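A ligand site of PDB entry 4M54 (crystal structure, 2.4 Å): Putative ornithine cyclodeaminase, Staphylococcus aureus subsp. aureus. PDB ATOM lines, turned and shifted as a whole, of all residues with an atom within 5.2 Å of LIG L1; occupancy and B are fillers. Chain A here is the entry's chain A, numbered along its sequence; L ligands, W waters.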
ATOM      1  N   LYS A  48      39.854   1.684 -25.306  1.00  0.00           N
ATOM      2  CA  LYS A  48      38.834   1.917 -24.295  1.00  0.00           C
ATOM      3  C   LYS A  48      39.246   1.362 -22.935  1.00  0.00           C
ATOM      4  O   LYS A  48      39.542   0.173 -22.803  1.00  0.00           O
ATOM      5  CB  LYS A  48      37.493   1.326 -24.740  1.00  0.00           C
ATOM      6  CG  LYS A  48      37.547  -0.146 -25.102  1.00  0.00           C
ATOM      7  CD  LYS A  48      36.456  -0.507 -26.077  1.00  0.00           C
ATOM      8  CE  LYS A  48      37.022  -1.345 -27.207  1.00  0.00           C
ATOM      9  NZ  LYS A  48      35.977  -1.711 -28.192  1.00  0.00           N
ATOM     10  N   TYR A  50      38.761   0.055 -19.156  1.00  0.00           N
ATOM     11  CA  TYR A  50      37.747  -0.639 -18.366  1.00  0.00           C
ATOM     12  C   TYR A  50      37.811  -0.170 -16.921  1.00  0.00           C
ATOM     13  O   TYR A  50      38.878  -0.079 -16.325  1.00  0.00           O
ATOM     14  CB  TYR A  50      37.974  -2.152 -18.424  1.00  0.00           C
ATOM     15  CG  TYR A  50      37.408  -2.819 -19.662  1.00  0.00           C
ATOM     16  CD1 TYR A  50      37.858  -2.475 -20.924  1.00  0.00           C
ATOM     17  CD2 TYR A  50      36.437  -3.808 -19.553  1.00  0.00           C
ATOM     18  CE1 TYR A  50      37.343  -3.083 -22.054  1.00  0.00           C
ATOM     19  CE2 TYR A  50      35.924  -4.429 -20.676  1.00  0.00           C
ATOM     20  CZ  TYR A  50      36.387  -4.062 -21.929  1.00  0.00           C
ATOM     21  OH  TYR A  50      35.881  -4.668 -23.057  1.00  0.00           O
ATOM     22  N   ARG A  63      31.431  -4.079 -14.995  1.00  0.00           N
ATOM     23  CA  ARG A  63      32.368  -3.033 -15.383  1.00  0.00           C
ATOM     24  C   ARG A  63      31.662  -1.832 -16.001  1.00  0.00           C
ATOM     25  O   ARG A  63      30.479  -1.910 -16.346  1.00  0.00           O
ATOM     26  CB  ARG A  63      33.405  -3.563 -16.378  1.00  0.00           C
ATOM     27  CG  ARG A  63      32.873  -3.753 -17.799  1.00  0.00           C
ATOM     28  CD  ARG A  63      32.023  -5.010 -17.933  1.00  0.00           C
ATOM     29  NE  ARG A  63      31.177  -4.988 -19.132  1.00  0.00           N
ATOM     30  CZ  ARG A  63      31.442  -5.656 -20.244  1.00  0.00           C
ATOM     31  NH1 ARG A  63      32.533  -6.403 -20.335  1.00  0.00           N
ATOM     32  NH2 ARG A  63      30.605  -5.575 -21.274  1.00  0.00           N
ATOM     33  N   ILE A  65      32.693   0.848 -19.192  1.00  0.00           N
ATOM     34  CA  ILE A  65      33.688   1.067 -20.230  1.00  0.00           C
ATOM     35  C   ILE A  65      33.551   2.431 -20.884  1.00  0.00           C
ATOM     36  O   ILE A  65      32.470   2.808 -21.341  1.00  0.00           O
ATOM     37  CB  ILE A  65      33.603  -0.017 -21.325  1.00  0.00           C
ATOM     38  CG1 ILE A  65      33.531  -1.409 -20.694  1.00  0.00           C
ATOM     39  CG2 ILE A  65      34.773   0.090 -22.284  1.00  0.00           C
ATOM     40  CD1 ILE A  65      33.201  -2.511 -21.673  1.00  0.00           C
ATOM     41  N   MET A  67      34.217   4.607 -24.004  1.00  0.00           N
ATOM     42  CA  MET A  67      34.501   4.384 -25.418  1.00  0.00           C
ATOM     43  C   MET A  67      34.441   5.671 -26.231  1.00  0.00           C
ATOM     44  O   MET A  67      33.416   5.975 -26.848  1.00  0.00           O
ATOM     45  CB  MET A  67      33.523   3.348 -25.992  1.00  0.00           C
ATOM     46  CG  MET A  67      33.576   1.998 -25.296  1.00  0.00           C
ATOM     47  SD  MET A  67      32.380   0.799 -25.929  1.00  0.00           S
ATOM     48  CE  MET A  67      32.892   0.681 -27.642  1.00  0.00           C
ATOM     49  N   LYS A  81      30.900   6.775 -25.526  1.00  0.00           N
ATOM     50  CA  LYS A  81      29.877   5.970 -24.881  1.00  0.00           C
ATOM     51  C   LYS A  81      30.385   5.552 -23.509  1.00  0.00           C
ATOM     52  O   LYS A  81      31.432   4.919 -23.385  1.00  0.00           O
ATOM     53  CB  LYS A  81      29.508   4.746 -25.724  1.00  0.00           C
ATOM     54  CG  LYS A  81      28.307   3.989 -25.169  1.00  0.00           C
ATOM     55  CD  LYS A  81      27.872   2.853 -26.082  1.00  0.00           C
ATOM     56  CE  LYS A  81      28.866   1.705 -26.052  1.00  0.00           C
ATOM     57  NZ  LYS A  81      28.386   0.554 -26.857  1.00  0.00           N
ATOM     58  N   ILE A  83      29.337   3.284 -20.867  1.00  0.00           N
ATOM     59  CA  ILE A  83      28.385   2.203 -20.661  1.00  0.00           C
ATOM     60  C   ILE A  83      28.775   1.253 -19.532  1.00  0.00           C
ATOM     61  O   ILE A  83      29.867   0.672 -19.525  1.00  0.00           O
ATOM     62  CB  ILE A  83      28.136   1.424 -21.981  1.00  0.00           C
ATOM     63  CG1 ILE A  83      27.123   0.300 -21.772  1.00  0.00           C
ATOM     64  CG2 ILE A  83      29.446   0.883 -22.560  1.00  0.00           C
ATOM     65  CD1 ILE A  83      26.579  -0.267 -23.058  1.00  0.00           C
ATOM     66  N   GLY A  84      27.881   1.120 -18.554  1.00  0.00           N
ATOM     67  CA  GLY A  84      28.131   0.279 -17.397  1.00  0.00           C
ATOM     68  C   GLY A  84      27.452  -1.066 -17.528  1.00  0.00           C
ATOM     69  O   GLY A  84      26.578  -1.250 -18.387  1.00  0.00           O
ATOM     70  N   SER A  85      27.852  -2.010 -16.682  1.00  0.00           N
ATOM     71  CA  SER A  85      27.293  -3.343 -16.728  1.00  0.00           C
ATOM     72  C   SER A  85      27.386  -4.061 -15.391  1.00  0.00           C
ATOM     73  O   SER A  85      28.372  -3.941 -14.663  1.00  0.00           O
ATOM     74  CB  SER A  85      27.987  -4.178 -17.807  1.00  0.00           C
ATOM     75  OG  SER A  85      27.517  -5.522 -17.798  1.00  0.00           O
ATOM     76  N   ARG A  97      21.050  -5.479 -17.649  1.00  0.00           N
ATOM     77  CA  ARG A  97      22.466  -5.630 -17.316  1.00  0.00           C
ATOM     78  C   ARG A  97      23.245  -4.371 -17.673  1.00  0.00           C
ATOM     79  O   ARG A  97      23.945  -3.804 -16.842  1.00  0.00           O
ATOM     80  CB  ARG A  97      23.059  -6.826 -18.058  1.00  0.00           C
ATOM     81  CG  ARG A  97      24.570  -6.937 -17.927  1.00  0.00           C
ATOM     82  CD  ARG A  97      25.153  -7.831 -19.000  1.00  0.00           C
ATOM     83  NE  ARG A  97      24.865  -7.317 -20.346  1.00  0.00           N
ATOM     84  CZ  ARG A  97      25.644  -6.457 -20.998  1.00  0.00           C
ATOM     85  NH1 ARG A  97      26.767  -6.018 -20.439  1.00  0.00           N
ATOM     86  NH2 ARG A  97      25.311  -6.044 -22.212  1.00  0.00           N
ATOM     87  N   ALA A  98      23.114  -3.946 -18.923  1.00  0.00           N
ATOM     88  CA  ALA A  98      23.848  -2.790 -19.413  1.00  0.00           C
ATOM     89  C   ALA A  98      23.022  -1.512 -19.335  1.00  0.00           C
ATOM     90  O   ALA A  98      21.804  -1.523 -19.511  1.00  0.00           O
ATOM     91  CB  ALA A  98      24.326  -3.023 -20.839  1.00  0.00           C
ATOM     92  N   SER A 122      23.275   0.970 -28.242  1.00  0.00           N
ATOM     93  CA  SER A 122      24.345  -0.025 -28.166  1.00  0.00           C
ATOM     94  C   SER A 122      23.901  -1.387 -28.691  1.00  0.00           C
ATOM     95  O   SER A 122      24.598  -2.015 -29.487  1.00  0.00           O
ATOM     96  CB  SER A 122      24.845  -0.152 -26.717  1.00  0.00           C
ATOM     97  OG  SER A 122      25.924  -1.072 -26.625  1.00  0.00           O
ATOM     98  N   ARG A 125      23.076  -1.169 -32.638  1.00  0.00           N
ATOM     99  CA  ARG A 125      24.233  -1.057 -33.523  1.00  0.00           C
ATOM    100  C   ARG A 125      24.986  -2.391 -33.571  1.00  0.00           C
ATOM    101  O   ARG A 125      25.552  -2.755 -34.602  1.00  0.00           O
ATOM    102  CB  ARG A 125      25.163   0.093 -33.113  1.00  0.00           C
ATOM    103  CG  ARG A 125      25.806   0.008 -31.715  1.00  0.00           C
ATOM    104  CD  ARG A 125      27.123  -0.771 -31.719  1.00  0.00           C
ATOM    105  NE  ARG A 125      28.003  -0.363 -30.624  1.00  0.00           N
ATOM    106  CZ  ARG A 125      29.066  -1.058 -30.223  1.00  0.00           C
ATOM    107  NH1 ARG A 125      29.367  -2.205 -30.798  1.00  0.00           N
ATOM    108  NH2 ARG A 125      29.813  -0.606 -29.228  1.00  0.00           N
ATOM    109  N   ILE A 238      29.272 -12.325 -31.266  1.00  0.00           N
ATOM    110  CA  ILE A 238      29.006 -11.080 -30.550  1.00  0.00           C
ATOM    111  C   ILE A 238      29.548 -11.090 -29.112  1.00  0.00           C
ATOM    112  O   ILE A 238      30.195 -10.134 -28.691  1.00  0.00           O
ATOM    113  CB  ILE A 238      27.489 -10.771 -30.519  1.00  0.00           C
ATOM    114  CG1 ILE A 238      26.963 -10.529 -31.941  1.00  0.00           C
ATOM    115  CG2 ILE A 238      27.196  -9.569 -29.629  1.00  0.00           C
ATOM    116  CD1 ILE A 238      27.623  -9.362 -32.644  1.00  0.00           C
ATOM    117  N   ILE A 240      31.862 -12.900 -27.976  1.00  0.00           N
ATOM    118  CA  ILE A 240      33.317 -13.098 -28.005  1.00  0.00           C
ATOM    119  C   ILE A 240      33.833 -14.423 -27.430  1.00  0.00           C
ATOM    120  O   ILE A 240      34.561 -15.154 -28.111  1.00  0.00           O
ATOM    121  CB  ILE A 240      34.072 -11.926 -27.324  1.00  0.00           C
ATOM    122  CG1 ILE A 240      33.786 -10.615 -28.069  1.00  0.00           C
ATOM    123  CG2 ILE A 240      35.565 -12.191 -27.279  1.00  0.00           C
ATOM    124  CD1 ILE A 240      34.262 -10.615 -29.500  1.00  0.00           C
ATOM    125  N   PRO A 309      33.797  -9.479 -33.545  1.00  0.00           N
ATOM    126  CA  PRO A 309      33.672  -8.033 -33.345  1.00  0.00           C
ATOM    127  C   PRO A 309      33.770  -7.623 -31.886  1.00  0.00           C
ATOM    128  O   PRO A 309      32.900  -7.967 -31.084  1.00  0.00           O
ATOM    129  CB  PRO A 309      32.272  -7.741 -33.894  1.00  0.00           C
ATOM    130  CG  PRO A 309      31.515  -9.059 -33.778  1.00  0.00           C
ATOM    131  CD  PRO A 309      32.491 -10.146 -33.410  1.00  0.00           C
ATOM    132  N   MET A 310      34.826  -6.895 -31.539  1.00  0.00           N
ATOM    133  CA  MET A 310      35.002  -6.407 -30.175  1.00  0.00           C
ATOM    134  C   MET A 310      34.039  -5.259 -29.865  1.00  0.00           C
ATOM    135  O   MET A 310      33.715  -5.010 -28.709  1.00  0.00           O
ATOM    136  CB  MET A 310      36.447  -5.953 -29.951  1.00  0.00           C
ATOM    137  CG  MET A 310      37.240  -6.827 -28.992  1.00  0.00           C
ATOM    138  SD  MET A 310      37.432  -8.525 -29.571  1.00  0.00           S
ATOM    139  CE  MET A 310      38.430  -9.207 -28.249  1.00  0.00           C
ATOM    140  N   GLY A 311      33.585  -4.577 -30.909  1.00  0.00           N
ATOM    141  CA  GLY A 311      32.718  -3.426 -30.750  1.00  0.00           C
ATOM    142  C   GLY A 311      33.528  -2.137 -30.756  1.00  0.00           C
ATOM    143  O   GLY A 311      34.494  -1.998 -30.003  1.00  0.00           O
ATOM    144  N   MET A 312      33.144  -1.205 -31.616  1.00  0.00           N
ATOM    145  CA  MET A 312      33.896   0.035 -31.769  1.00  0.00           C
ATOM    146  C   MET A 312      33.077   1.257 -31.372  1.00  0.00           C
ATOM    147  O   MET A 312      31.869   1.301 -31.570  1.00  0.00           O
ATOM    148  CB  MET A 312      34.395   0.188 -33.210  1.00  0.00           C
ATOM    149  CG  MET A 312      35.351  -0.899 -33.649  1.00  0.00           C
ATOM    150  SD  MET A 312      36.001  -0.638 -35.308  1.00  0.00           S
ATOM    151  CE  MET A 312      34.485  -0.652 -36.255  1.00  0.00           C
ATOM    152  N   ASP A 316      28.895   3.506 -32.073  1.00  0.00           N
ATOM    153  CA  ASP A 316      27.942   4.126 -31.169  1.00  0.00           C
ATOM    154  C   ASP A 316      27.774   5.603 -31.490  1.00  0.00           C
ATOM    155  O   ASP A 316      26.663   6.130 -31.485  1.00  0.00           O
ATOM    156  CB  ASP A 316      28.396   3.970 -29.711  1.00  0.00           C
ATOM    157  CG  ASP A 316      28.801   2.547 -29.389  1.00  0.00           C
ATOM    158  OD1 ASP A 316      27.895   1.701 -29.216  1.00  0.00           O
ATOM    159  OD2 ASP A 316      30.014   2.270 -29.280  1.00  0.00           O
HETATM  160  O1  LIG L   1      26.541  -3.767 -23.156  1.00  0.00           O
HETATM  161  C1  LIG L   1      27.791  -3.629 -23.136  1.00  0.00           C
HETATM  162  O2  LIG L   1      28.444  -3.953 -22.116  1.00  0.00           O
HETATM  163  C2  LIG L   1      28.504  -3.079 -24.365  1.00  0.00           C
HETATM  164  C3  LIG L   1      29.992  -3.265 -24.229  1.00  0.00           C
HETATM  165  C4  LIG L   1      30.582  -3.679 -25.593  1.00  0.00           C
HETATM  166  N1  LIG L   1      31.881  -4.196 -25.402  1.00  0.00           N
HETATM  167  C5  LIG L   1      31.785  -5.573 -24.979  1.00  0.00           C
HETATM  168  C6  LIG L   1      33.130  -6.275 -25.230  1.00  0.00           C
HETATM  169  N2  LIG L   1      33.015  -7.109 -26.379  1.00  0.00           N
HETATM  170  C7  LIG L   1      33.490  -7.127 -24.027  1.00  0.00           C
HETATM  171  O3  LIG L   1      33.953  -6.587 -22.977  1.00  0.00           O
HETATM  172  O4  LIG L   1      33.335  -8.360 -24.077  1.00  0.00           O
HETATM  173  C8  LIG L   1      30.651  -2.490 -26.516  1.00  0.00           C
HETATM  174  O5  LIG L   1      31.342  -2.559 -27.587  1.00  0.00           O
HETATM  175  O6  LIG L   1      30.020  -1.420 -26.243  1.00  0.00           O
HETATM  176  P1  LG2 L   2      21.984 -10.569 -20.474  1.00  0.00           P
HETATM  177  O1  LG2 L   2      22.568 -10.944 -19.125  1.00  0.00           O
HETATM  178  O2  LG2 L   2      20.604  -9.970 -20.282  1.00  0.00           O
HETATM  179  O3  LG2 L   2      21.901 -11.871 -21.400  1.00  0.00           O
HETATM  180  C1  LG2 L   2      22.575 -13.051 -20.946  1.00  0.00           C
HETATM  181  C2  LG2 L   2      21.785 -14.259 -21.345  1.00  0.00           C
HETATM  182  O4  LG2 L   2      22.683 -15.242 -21.995  1.00  0.00           O
HETATM  183  C3  LG2 L   2      21.204 -14.888 -20.146  1.00  0.00           C
HETATM  184  O5  LG2 L   2      19.840 -15.295 -20.434  1.00  0.00           O
HETATM  185  C4  LG2 L   2      22.023 -16.069 -19.884  1.00  0.00           C
HETATM  186  O6  LG2 L   2      21.251 -17.104 -19.228  1.00  0.00           O
HETATM  187  C5  LG2 L   2      22.435 -16.495 -21.221  1.00  0.00           C
HETATM  188  N1  LG2 L   2      23.574 -17.302 -21.182  1.00  0.00           N
HETATM  189  C6  LG2 L   2      24.656 -17.152 -20.449  1.00  0.00           C
HETATM  190  N2  LG2 L   2      25.536 -17.857 -20.476  1.00  0.00           N
HETATM  191  C7  LG2 L   2      25.554 -18.755 -21.152  1.00  0.00           C
HETATM  192  C8  LG2 L   2      26.164 -19.986 -21.735  1.00  0.00           C
HETATM  193  N3  LG2 L   2      27.476 -20.339 -21.255  1.00  0.00           N
HETATM  194  N4  LG2 L   2      25.674 -20.728 -22.592  1.00  0.00           N
HETATM  195  C9  LG2 L   2      24.645 -20.596 -23.088  1.00  0.00           C
HETATM  196  N5  LG2 L   2      23.847 -19.700 -22.853  1.00  0.00           N
HETATM  197  C10 LG2 L   2      24.055 -18.650 -21.941  1.00  0.00           C
HETATM  198  O7  LG2 L   2      22.912  -9.479 -21.144  1.00  0.00           O
HETATM  199  P2  LG2 L   2      22.873  -9.105 -22.691  1.00  0.00           P
HETATM  200  O8  LG2 L   2      22.927  -7.598 -22.808  1.00  0.00           O
HETATM  201  O9  LG2 L   2      21.609  -9.624 -23.350  1.00  0.00           O
HETATM  202  O10 LG2 L   2      24.146  -9.759 -23.438  1.00  0.00           O
HETATM  203  C11 LG2 L   2      25.374  -9.039 -23.369  1.00  0.00           C
HETATM  204  C12 LG2 L   2      26.475  -9.844 -23.956  1.00  0.00           C
HETATM  205  O11 LG2 L   2      26.724  -9.408 -25.369  1.00  0.00           O
HETATM  206  C13 LG2 L   2      27.689  -9.588 -23.178  1.00  0.00           C
HETATM  207  O12 LG2 L   2      28.540 -10.773 -23.180  1.00  0.00           O
HETATM  208  C14 LG2 L   2      28.351  -8.509 -23.880  1.00  0.00           C
HETATM  209  O13 LG2 L   2      29.781  -8.473 -23.566  1.00  0.00           O
HETATM  210  C15 LG2 L   2      28.120  -8.846 -25.290  1.00  0.00           C
HETATM  211  N6  LG2 L   2      28.289  -7.734 -26.117  1.00  0.00           N
HETATM  212  C16 LG2 L   2      29.132  -7.449 -27.174  1.00  0.00           C
HETATM  213  C17 LG2 L   2      28.969  -6.314 -27.929  1.00  0.00           C
HETATM  214  C18 LG2 L   2      29.956  -6.087 -29.070  1.00  0.00           C
HETATM  215  O14 LG2 L   2      30.060  -4.982 -29.596  1.00  0.00           O
HETATM  216  N7  LG2 L   2      30.758  -7.174 -29.529  1.00  0.00           N
HETATM  217  C19 LG2 L   2      27.811  -5.269 -27.666  1.00  0.00           C
HETATM  218  C20 LG2 L   2      27.113  -5.629 -26.329  1.00  0.00           C
HETATM  219  C21 LG2 L   2      27.357  -6.796 -25.633  1.00  0.00           C
HETATM  220  O   HOH W   1      25.008  -3.099 -25.184  1.00  0.00           O
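O of Lys 81 lies within hydrogen-bond range of N of Met 67, 2.9 Å away.
NH1 of Arg 97 lies within hydrogen-bond range of OG of Ser 85, at 2.8 Å.
The side-chain amino group of Lys 81 is in hydrogen-bond range of the side-chain hydroxyl of Ser 122, 3.0 Å away.
O of Arg 63 is in hydrogen-bond range of N of Ser 85, at 2.7 Å.
N of Ile 65 lies within hydrogen-bond range of O of Ile 83.
NE of Arg 125 lies within salt-bridge range of OD1 of Asp 316, 2.5 Å away.
The side-chain amino group (NZ) of Lys 81 lies within salt-bridge range of the side-chain carboxylate (OD1) of Asp 316 (2.7 Å).
A nitrogen (N7) of LG2 L2 sits at hydrogen-bond distance from the backbone carbonyl oxygen (O) of Pro 309, at 2.8 Å.
The guanidinium group (NH2) of Arg 97 is in salt-bridge range of an oxygen (O1) of LIG L1.
NH1 of Arg 125 sits at hydrogen-bond distance from O14 of LG2 L2 (3.1 Å).
NH2 of Arg 63 is in salt-bridge range of O2 of LIG L1 (2.8 Å).
An oxygen (O6) of LIG L1 is in salt-bridge range of the side-chain amino group of Lys 81 (2.6 Å).
NH2 of Arg 97 is in salt-bridge range of O8 of LG2 L2, at 2.9 Å.
O5 of LIG L1 lies within salt-bridge range of NH2 of Arg 125 (3.0 Å).
O3 of LIG L1 lies within hydrogen-bond range of OH of Tyr 50.
O of Met 310 sits at hydrogen-bond distance from N2 of LIG L1, at 3.2 Å.
A nitrogen (N7) of LG2 L2 lies within hydrogen-bond range of the backbone carbonyl oxygen (O) of Ile 238 (3.1 Å).
SD of Met 67 lies close to O6 of LIG L1.
Merely in contact with LIG L1: Ile 83, Ala 98, Ser 122, Ile 240 and Gly 311.
Hydrophobic or aromatic side chains within 4 Å of LIG L1: Tyr 50, Met 67, Ile 83, Ala 98 and Ile 240.
Within 4 Å of LIG L1: Tyr 50, Arg 63, Met 67, Lys 81, Ile 83, Arg 97, Ala 98, Ser 122, Arg 125, Ile 240, Met 310 and Gly 311.
Along chain A the residues within 4 Å of LIG L1 span positions 50 to 311.
Water W1 bridges O1 of LIG L1 and OG of Ser 122.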
